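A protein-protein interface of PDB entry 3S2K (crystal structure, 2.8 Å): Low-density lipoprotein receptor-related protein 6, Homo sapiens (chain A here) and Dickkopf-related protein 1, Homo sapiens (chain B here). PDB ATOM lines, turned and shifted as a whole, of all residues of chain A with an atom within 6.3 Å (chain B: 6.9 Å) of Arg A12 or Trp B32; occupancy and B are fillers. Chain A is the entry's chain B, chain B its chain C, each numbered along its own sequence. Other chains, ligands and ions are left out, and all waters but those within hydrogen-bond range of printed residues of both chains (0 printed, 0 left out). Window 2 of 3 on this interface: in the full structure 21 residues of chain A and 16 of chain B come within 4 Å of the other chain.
NH1 of Arg A12 sits close to NE1 of Trp B32, at 3.5 Å.
The backbone NH of Met A250 lies within hydrogen-bond range of the backbone carbonyl oxygen of Ser A10 (3.1 Å). The side-chain hydroxyl (OG) of Ser A10 sits at hydrogen-bond distance from the backbone carbonyl oxygen (O) of Ser A38. The guanidinium group of Arg A12 lies within salt-bridge range of the side-chain carboxylate of Glu A36 (2.5 Å). O of Glu A36 lies within hydrogen-bond range of N of Ile A54 (3.1 Å). The backbone NH (N) of Phe B31 sits at hydrogen-bond distance from the backbone carbonyl oxygen (O) of Ile B59 (2.8 Å). The backbone NH of Glu A36 sits at hydrogen-bond distance from the side-chain carboxylate of Asp A53, 3.0 Å away.
Among the printed residues, merely in contact across the chains: Glu A36 with Trp B32 (3.2 Å), Ser A38 with Phe B31 (3.9 Å), Ile A54 with Phe B31 (3.6 Å), Trp A223 with Ile B59 (3.4 Å), Met A250 with Trp B32 (3.8 Å) and Met A250 with Ile B59 (3.9 Å).
Arg A12 touches just one residue of chain B: Trp B32 (3.4 Å). Of the printed residues of chain B, Glu A36 touches Trp B32. Printed residues of chain B within 4 Å of Trp A223: Ile B59 (3.4 Å). Trp B32 touches just these residues of chain A: Arg A12 (3.4 Å), Glu A36 (3.2 Å) and Met A250 (3.8 Å). Of the printed residues of chain A, Ile B59 touches Trp A223 (3.4 Å) and Met A250 (3.9 Å). The nearest printed residue of chain B that does not touch Arg A12 is Phe B31 (6.9 Å).
Of the 17 printed residues of chain A, 6 touch a printed residue of chain B. Printed residues of chain A that touch a printed residue of chain B: Arg A12, Glu A36, Ser A38, Ile A54, Trp A223 and Met A250. Along chain A the printed residues that touch a printed residue of chain B span positions 12 to 250. Hydrophobic or aromatic side chains of chain B that line the printed part of chain A: Phe B31, Trp B32 and Ile B59. Among the printed residues, 7 pairs touch across the chains. Among the printed residues, no Asp or Glu carboxylate lies within 4 Å of a Lys or Arg side-chain nitrogen of the other chain.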
ATOM      1  N   SER A  10     -12.598  19.498  -2.696  1.00  0.00           N
ATOM      2  CA  SER A  10     -13.475  20.649  -2.878  1.00  0.00           C
ATOM      3  C   SER A  10     -13.045  21.770  -1.946  1.00  0.00           C
ATOM      4  O   SER A  10     -12.507  21.516  -0.865  1.00  0.00           O
ATOM      5  CB  SER A  10     -14.935  20.273  -2.620  1.00  0.00           C
ATOM      6  OG  SER A  10     -15.136  19.880  -1.273  1.00  0.00           O
ATOM      7  N   ARG A  11     -13.279  23.010  -2.363  1.00  0.00           N
ATOM      8  CA  ARG A  11     -12.847  24.152  -1.569  1.00  0.00           C
ATOM      9  C   ARG A  11     -13.685  25.388  -1.860  1.00  0.00           C
ATOM     10  O   ARG A  11     -13.217  26.342  -2.485  1.00  0.00           O
ATOM     11  CB  ARG A  11     -11.367  24.438  -1.815  1.00  0.00           C
ATOM     12  CG  ARG A  11     -10.779  25.470  -0.884  1.00  0.00           C
ATOM     13  CD  ARG A  11      -9.418  25.918  -1.369  1.00  0.00           C
ATOM     14  NE  ARG A  11      -9.076  27.237  -0.850  1.00  0.00           N
ATOM     15  CZ  ARG A  11      -9.495  28.377  -1.391  1.00  0.00           C
ATOM     16  NH1 ARG A  11     -10.275  28.357  -2.465  1.00  0.00           N
ATOM     17  NH2 ARG A  11      -9.139  29.536  -0.857  1.00  0.00           N
ATOM     18  N   ARG A  12     -14.932  25.354  -1.404  1.00  0.00           N
ATOM     19  CA  ARG A  12     -15.857  26.470  -1.557  1.00  0.00           C
ATOM     20  C   ARG A  12     -16.086  26.865  -3.015  1.00  0.00           C
ATOM     21  O   ARG A  12     -16.889  26.250  -3.713  1.00  0.00           O
ATOM     22  CB  ARG A  12     -15.390  27.669  -0.731  1.00  0.00           C
ATOM     23  CG  ARG A  12     -15.291  27.362   0.750  1.00  0.00           C
ATOM     24  CD  ARG A  12     -15.006  28.610   1.566  1.00  0.00           C
ATOM     25  NE  ARG A  12     -16.162  29.499   1.655  1.00  0.00           N
ATOM     26  CZ  ARG A  12     -16.186  30.617   2.373  1.00  0.00           C
ATOM     27  NH1 ARG A  12     -15.116  30.982   3.069  1.00  0.00           N
ATOM     28  NH2 ARG A  12     -17.278  31.371   2.399  1.00  0.00           N
ATOM     29  N   ALA A  13     -15.377  27.888  -3.472  1.00  0.00           N
ATOM     30  CA  ALA A  13     -15.600  28.421  -4.812  1.00  0.00           C
ATOM     31  C   ALA A  13     -15.027  27.534  -5.917  1.00  0.00           C
ATOM     32  O   ALA A  13     -15.409  27.665  -7.077  1.00  0.00           O
ATOM     33  CB  ALA A  13     -15.044  29.837  -4.919  1.00  0.00           C
ATOM     34  N   ASP A  14     -14.115  26.635  -5.564  1.00  0.00           N
ATOM     35  CA  ASP A  14     -13.472  25.800  -6.577  1.00  0.00           C
ATOM     36  C   ASP A  14     -13.093  24.392  -6.109  1.00  0.00           C
ATOM     37  O   ASP A  14     -13.012  24.115  -4.910  1.00  0.00           O
ATOM     38  CB  ASP A  14     -12.254  26.516  -7.184  1.00  0.00           C
ATOM     39  CG  ASP A  14     -11.315  27.082  -6.131  1.00  0.00           C
ATOM     40  OD1 ASP A  14     -11.055  26.394  -5.121  1.00  0.00           O
ATOM     41  OD2 ASP A  14     -10.834  28.221  -6.317  1.00  0.00           O
ATOM     42  N   ILE A  15     -12.880  23.509  -7.080  1.00  0.00           N
ATOM     43  CA  ILE A  15     -12.422  22.146  -6.833  1.00  0.00           C
ATOM     44  C   ILE A  15     -11.046  21.990  -7.472  1.00  0.00           C
ATOM     45  O   ILE A  15     -10.850  22.363  -8.629  1.00  0.00           O
ATOM     46  CB  ILE A  15     -13.399  21.120  -7.435  1.00  0.00           C
ATOM     47  CG1 ILE A  15     -14.803  21.333  -6.860  1.00  0.00           C
ATOM     48  CG2 ILE A  15     -12.911  19.699  -7.187  1.00  0.00           C
ATOM     49  CD1 ILE A  15     -15.867  20.456  -7.488  1.00  0.00           C
ATOM     50  N   VAL A  34     -19.564  27.930  -9.761  1.00  0.00           N
ATOM     51  CA  VAL A  34     -19.510  27.215  -8.493  1.00  0.00           C
ATOM     52  C   VAL A  34     -19.474  28.209  -7.341  1.00  0.00           C
ATOM     53  O   VAL A  34     -18.598  29.072  -7.280  1.00  0.00           O
ATOM     54  CB  VAL A  34     -18.291  26.278  -8.402  1.00  0.00           C
ATOM     55  CG1 VAL A  34     -18.226  25.637  -7.028  1.00  0.00           C
ATOM     56  CG2 VAL A  34     -18.349  25.213  -9.491  1.00  0.00           C
ATOM     57  N   LYS A  35     -20.436  28.088  -6.433  1.00  0.00           N
ATOM     58  CA  LYS A  35     -20.534  29.010  -5.311  1.00  0.00           C
ATOM     59  C   LYS A  35     -19.954  28.416  -4.028  1.00  0.00           C
ATOM     60  O   LYS A  35     -19.051  28.996  -3.422  1.00  0.00           O
ATOM     61  CB  LYS A  35     -21.986  29.451  -5.101  1.00  0.00           C
ATOM     62  CG  LYS A  35     -22.539  30.301  -6.231  1.00  0.00           C
ATOM     63  CD  LYS A  35     -21.681  31.537  -6.454  1.00  0.00           C
ATOM     64  CE  LYS A  35     -22.211  32.393  -7.595  1.00  0.00           C
ATOM     65  NZ  LYS A  35     -22.265  31.646  -8.883  1.00  0.00           N
ATOM     66  N   GLU A  36     -20.464  27.258  -3.623  1.00  0.00           N
ATOM     67  CA  GLU A  36     -20.009  26.623  -2.391  1.00  0.00           C
ATOM     68  C   GLU A  36     -20.005  25.102  -2.514  1.00  0.00           C
ATOM     69  O   GLU A  36     -20.941  24.431  -2.087  1.00  0.00           O
ATOM     70  CB  GLU A  36     -20.891  27.046  -1.219  1.00  0.00           C
ATOM     71  CG  GLU A  36     -20.142  27.197   0.086  1.00  0.00           C
ATOM     72  CD  GLU A  36     -19.312  28.463   0.128  1.00  0.00           C
ATOM     73  OE1 GLU A  36     -19.844  29.530  -0.239  1.00  0.00           O
ATOM     74  OE2 GLU A  36     -18.130  28.390   0.525  1.00  0.00           O
ATOM     75  N   ALA A  37     -18.942  24.566  -3.104  1.00  0.00           N
ATOM     76  CA  ALA A  37     -18.807  23.125  -3.295  1.00  0.00           C
ATOM     77  C   ALA A  37     -18.549  22.431  -1.966  1.00  0.00           C
ATOM     78  O   ALA A  37     -17.729  22.893  -1.168  1.00  0.00           O
ATOM     79  CB  ALA A  37     -17.691  22.820  -4.288  1.00  0.00           C
ATOM     80  N   SER A  38     -19.256  21.332  -1.719  1.00  0.00           N
ATOM     81  CA  SER A  38     -19.059  20.589  -0.481  1.00  0.00           C
ATOM     82  C   SER A  38     -18.726  19.124  -0.764  1.00  0.00           C
ATOM     83  O   SER A  38     -17.560  18.763  -0.871  1.00  0.00           O
ATOM     84  CB  SER A  38     -20.280  20.710   0.434  1.00  0.00           C
ATOM     85  OG  SER A  38     -20.037  20.091   1.684  1.00  0.00           O
ATOM     86  N   ASP A  53     -23.370  21.604  -4.183  1.00  0.00           N
ATOM     87  CA  ASP A  53     -23.196  23.012  -3.859  1.00  0.00           C
ATOM     88  C   ASP A  53     -24.292  23.429  -2.883  1.00  0.00           C
ATOM     89  O   ASP A  53     -25.466  23.495  -3.245  1.00  0.00           O
ATOM     90  CB  ASP A  53     -23.236  23.858  -5.135  1.00  0.00           C
ATOM     91  CG  ASP A  53     -22.850  25.303  -4.889  1.00  0.00           C
ATOM     92  OD1 ASP A  53     -23.271  25.866  -3.854  1.00  0.00           O
ATOM     93  OD2 ASP A  53     -22.124  25.872  -5.734  1.00  0.00           O
ATOM     94  N   ILE A  54     -23.908  23.689  -1.638  1.00  0.00           N
ATOM     95  CA  ILE A  54     -24.890  23.950  -0.589  1.00  0.00           C
ATOM     96  C   ILE A  54     -25.394  25.394  -0.605  1.00  0.00           C
ATOM     97  O   ILE A  54     -26.250  25.776   0.192  1.00  0.00           O
ATOM     98  CB  ILE A  54     -24.363  23.543   0.812  1.00  0.00           C
ATOM     99  CG1 ILE A  54     -23.102  24.326   1.181  1.00  0.00           C
ATOM    100  CG2 ILE A  54     -24.088  22.051   0.857  1.00  0.00           C
ATOM    101  CD1 ILE A  54     -23.377  25.664   1.816  1.00  0.00           C
ATOM    102  N   TRP A 223      -8.557  22.070   9.570  1.00  0.00           N
ATOM    103  CA  TRP A 223      -8.992  23.455   9.486  1.00  0.00           C
ATOM    104  C   TRP A 223      -8.106  24.403  10.288  1.00  0.00           C
ATOM    105  O   TRP A 223      -7.955  25.573   9.931  1.00  0.00           O
ATOM    106  CB  TRP A 223     -10.441  23.572   9.959  1.00  0.00           C
ATOM    107  CG  TRP A 223     -11.448  23.328   8.886  1.00  0.00           C
ATOM    108  CD1 TRP A 223     -11.521  22.249   8.053  1.00  0.00           C
ATOM    109  CD2 TRP A 223     -12.543  24.176   8.538  1.00  0.00           C
ATOM    110  NE1 TRP A 223     -12.591  22.379   7.203  1.00  0.00           N
ATOM    111  CE2 TRP A 223     -13.236  23.557   7.482  1.00  0.00           C
ATOM    112  CE3 TRP A 223     -13.002  25.409   9.015  1.00  0.00           C
ATOM    113  CZ2 TRP A 223     -14.362  24.123   6.893  1.00  0.00           C
ATOM    114  CZ3 TRP A 223     -14.120  25.970   8.431  1.00  0.00           C
ATOM    115  CH2 TRP A 223     -14.787  25.328   7.381  1.00  0.00           C
ATOM    116  N   ASP A 247      -7.013  27.069   3.018  1.00  0.00           N
ATOM    117  CA  ASP A 247      -8.150  27.487   3.832  1.00  0.00           C
ATOM    118  C   ASP A 247      -9.439  26.789   3.403  1.00  0.00           C
ATOM    119  O   ASP A 247      -9.749  26.720   2.211  1.00  0.00           O
ATOM    120  CB  ASP A 247      -8.334  29.007   3.760  1.00  0.00           C
ATOM    121  CG  ASP A 247      -7.063  29.767   4.087  1.00  0.00           C
ATOM    122  OD1 ASP A 247      -6.274  30.038   3.156  1.00  0.00           O
ATOM    123  OD2 ASP A 247      -6.856  30.097   5.274  1.00  0.00           O
ATOM    124  N   TYR A 248     -10.174  26.271   4.385  1.00  0.00           N
ATOM    125  CA  TYR A 248     -11.503  25.707   4.167  1.00  0.00           C
ATOM    126  C   TYR A 248     -11.530  24.578   3.132  1.00  0.00           C
ATOM    127  O   TYR A 248     -12.188  24.696   2.094  1.00  0.00           O
ATOM    128  CB  TYR A 248     -12.489  26.804   3.742  1.00  0.00           C
ATOM    129  CG  TYR A 248     -12.376  28.103   4.514  1.00  0.00           C
ATOM    130  CD1 TYR A 248     -12.222  28.112   5.896  1.00  0.00           C
ATOM    131  CD2 TYR A 248     -12.424  29.325   3.853  1.00  0.00           C
ATOM    132  CE1 TYR A 248     -12.121  29.304   6.597  1.00  0.00           C
ATOM    133  CE2 TYR A 248     -12.323  30.519   4.542  1.00  0.00           C
ATOM    134  CZ  TYR A 248     -12.171  30.504   5.912  1.00  0.00           C
ATOM    135  OH  TYR A 248     -12.071  31.697   6.596  1.00  0.00           O
ATOM    136  N   MET A 250     -13.073  21.418   2.144  1.00  0.00           N
ATOM    137  CA  MET A 250     -14.300  20.737   2.527  1.00  0.00           C
ATOM    138  C   MET A 250     -14.186  19.214   2.450  1.00  0.00           C
ATOM    139  O   MET A 250     -14.164  18.537   3.476  1.00  0.00           O
ATOM    140  CB  MET A 250     -15.480  21.257   1.696  1.00  0.00           C
ATOM    141  CG  MET A 250     -15.618  22.776   1.745  1.00  0.00           C
ATOM    142  SD  MET A 250     -15.307  23.447   3.398  1.00  0.00           S
ATOM    143  CE  MET A 250     -16.587  22.663   4.368  1.00  0.00           C
ATOM    144  N   ARG B  29     -24.851  28.932  13.315  1.00  0.00           N
ATOM    145  CA  ARG B  29     -24.343  28.968  11.949  1.00  0.00           C
ATOM    146  C   ARG B  29     -24.177  27.576  11.352  1.00  0.00           C
ATOM    147  O   ARG B  29     -23.741  26.642  12.023  1.00  0.00           O
ATOM    148  CB  ARG B  29     -23.055  29.793  11.828  1.00  0.00           C
ATOM    149  CG  ARG B  29     -21.904  29.352  12.705  1.00  0.00           C
ATOM    150  CD  ARG B  29     -20.703  30.272  12.503  1.00  0.00           C
ATOM    151  NE  ARG B  29     -19.604  29.965  13.414  1.00  0.00           N
ATOM    152  CZ  ARG B  29     -19.424  30.547  14.597  1.00  0.00           C
ATOM    153  NH1 ARG B  29     -20.274  31.473  15.021  1.00  0.00           N
ATOM    154  NH2 ARG B  29     -18.394  30.201  15.357  1.00  0.00           N
ATOM    155  N   HIS B  30     -24.571  27.453  10.091  1.00  0.00           N
ATOM    156  CA  HIS B  30     -24.378  26.235   9.319  1.00  0.00           C
ATOM    157  C   HIS B  30     -23.704  26.630   8.017  1.00  0.00           C
ATOM    158  O   HIS B  30     -24.300  27.304   7.175  1.00  0.00           O
ATOM    159  CB  HIS B  30     -25.711  25.540   9.042  1.00  0.00           C
ATOM    160  CG  HIS B  30     -25.568  24.097   8.665  1.00  0.00           C
ATOM    161  ND1 HIS B  30     -25.025  23.161   9.516  1.00  0.00           N
ATOM    162  CD2 HIS B  30     -25.892  23.437   7.529  1.00  0.00           C
ATOM    163  CE1 HIS B  30     -25.023  21.979   8.921  1.00  0.00           C
ATOM    164  NE2 HIS B  30     -25.542  22.118   7.717  1.00  0.00           N
ATOM    165  N   PHE B  31     -22.454  26.213   7.866  1.00  0.00           N
ATOM    166  CA  PHE B  31     -21.608  26.688   6.779  1.00  0.00           C
ATOM    167  C   PHE B  31     -21.381  28.194   6.900  1.00  0.00           C
ATOM    168  O   PHE B  31     -20.803  28.653   7.886  1.00  0.00           O
ATOM    169  CB  PHE B  31     -22.176  26.299   5.412  1.00  0.00           C
ATOM    170  CG  PHE B  31     -22.054  24.828   5.099  1.00  0.00           C
ATOM    171  CD1 PHE B  31     -20.845  24.292   4.672  1.00  0.00           C
ATOM    172  CD2 PHE B  31     -23.148  23.982   5.228  1.00  0.00           C
ATOM    173  CE1 PHE B  31     -20.729  22.941   4.380  1.00  0.00           C
ATOM    174  CE2 PHE B  31     -23.040  22.627   4.936  1.00  0.00           C
ATOM    175  CZ  PHE B  31     -21.828  22.109   4.511  1.00  0.00           C
ATOM    176  N   TRP B  32     -21.837  28.967   5.919  1.00  0.00           N
ATOM    177  CA  TRP B  32     -21.541  30.401   5.921  1.00  0.00           C
ATOM    178  C   TRP B  32     -22.760  31.317   6.014  1.00  0.00           C
ATOM    179  O   TRP B  32     -22.745  32.449   5.532  1.00  0.00           O
ATOM    180  CB  TRP B  32     -20.632  30.767   4.749  1.00  0.00           C
ATOM    181  CG  TRP B  32     -19.298  30.106   4.899  1.00  0.00           C
ATOM    182  CD1 TRP B  32     -18.229  30.566   5.615  1.00  0.00           C
ATOM    183  CD2 TRP B  32     -18.904  28.839   4.360  1.00  0.00           C
ATOM    184  NE1 TRP B  32     -17.188  29.672   5.540  1.00  0.00           N
ATOM    185  CE2 TRP B  32     -17.576  28.603   4.775  1.00  0.00           C
ATOM    186  CE3 TRP B  32     -19.540  27.887   3.558  1.00  0.00           C
ATOM    187  CZ2 TRP B  32     -16.876  27.457   4.415  1.00  0.00           C
ATOM    188  CZ3 TRP B  32     -18.843  26.748   3.202  1.00  0.00           C
ATOM    189  CH2 TRP B  32     -17.524  26.542   3.630  1.00  0.00           C
ATOM    190  N   SER B  33     -23.803  30.809   6.655  1.00  0.00           N
ATOM    191  CA  SER B  33     -24.963  31.602   7.033  1.00  0.00           C
ATOM    192  C   SER B  33     -25.499  30.993   8.319  1.00  0.00           C
ATOM    193  O   SER B  33     -24.962  29.999   8.808  1.00  0.00           O
ATOM    194  CB  SER B  33     -26.031  31.580   5.937  1.00  0.00           C
ATOM    195  OG  SER B  33     -26.466  30.257   5.670  1.00  0.00           O
ATOM    196  N   LYS B  34     -26.550  31.579   8.874  1.00  0.00           N
ATOM    197  CA  LYS B  34     -27.127  31.041  10.096  1.00  0.00           C
ATOM    198  C   LYS B  34     -28.562  30.586   9.877  1.00  0.00           C
ATOM    199  O   LYS B  34     -29.329  31.235   9.168  1.00  0.00           O
ATOM    200  CB  LYS B  34     -27.051  32.068  11.225  1.00  0.00           C
ATOM    201  CG  LYS B  34     -25.632  32.408  11.644  1.00  0.00           C
ATOM    202  CD  LYS B  34     -25.610  33.458  12.744  1.00  0.00           C
ATOM    203  CE  LYS B  34     -24.182  33.802  13.136  1.00  0.00           C
ATOM    204  NZ  LYS B  34     -24.134  34.865  14.172  1.00  0.00           N
ATOM    205  N   ILE B  59     -18.075  25.880  11.807  1.00  0.00           N
ATOM    206  CA  ILE B  59     -19.108  26.232  10.833  1.00  0.00           C
ATOM    207  C   ILE B  59     -20.328  25.332  10.999  1.00  0.00           C
ATOM    208  O   ILE B  59     -21.366  25.554  10.378  1.00  0.00           O
ATOM    209  CB  ILE B  59     -18.604  26.137   9.376  1.00  0.00           C
ATOM    210  CG1 ILE B  59     -18.283  24.688   9.013  1.00  0.00           C
ATOM    211  CG2 ILE B  59     -17.391  27.026   9.165  1.00  0.00           C
ATOM    212  CD1 ILE B  59     -18.027  24.480   7.538  1.00  0.00           C
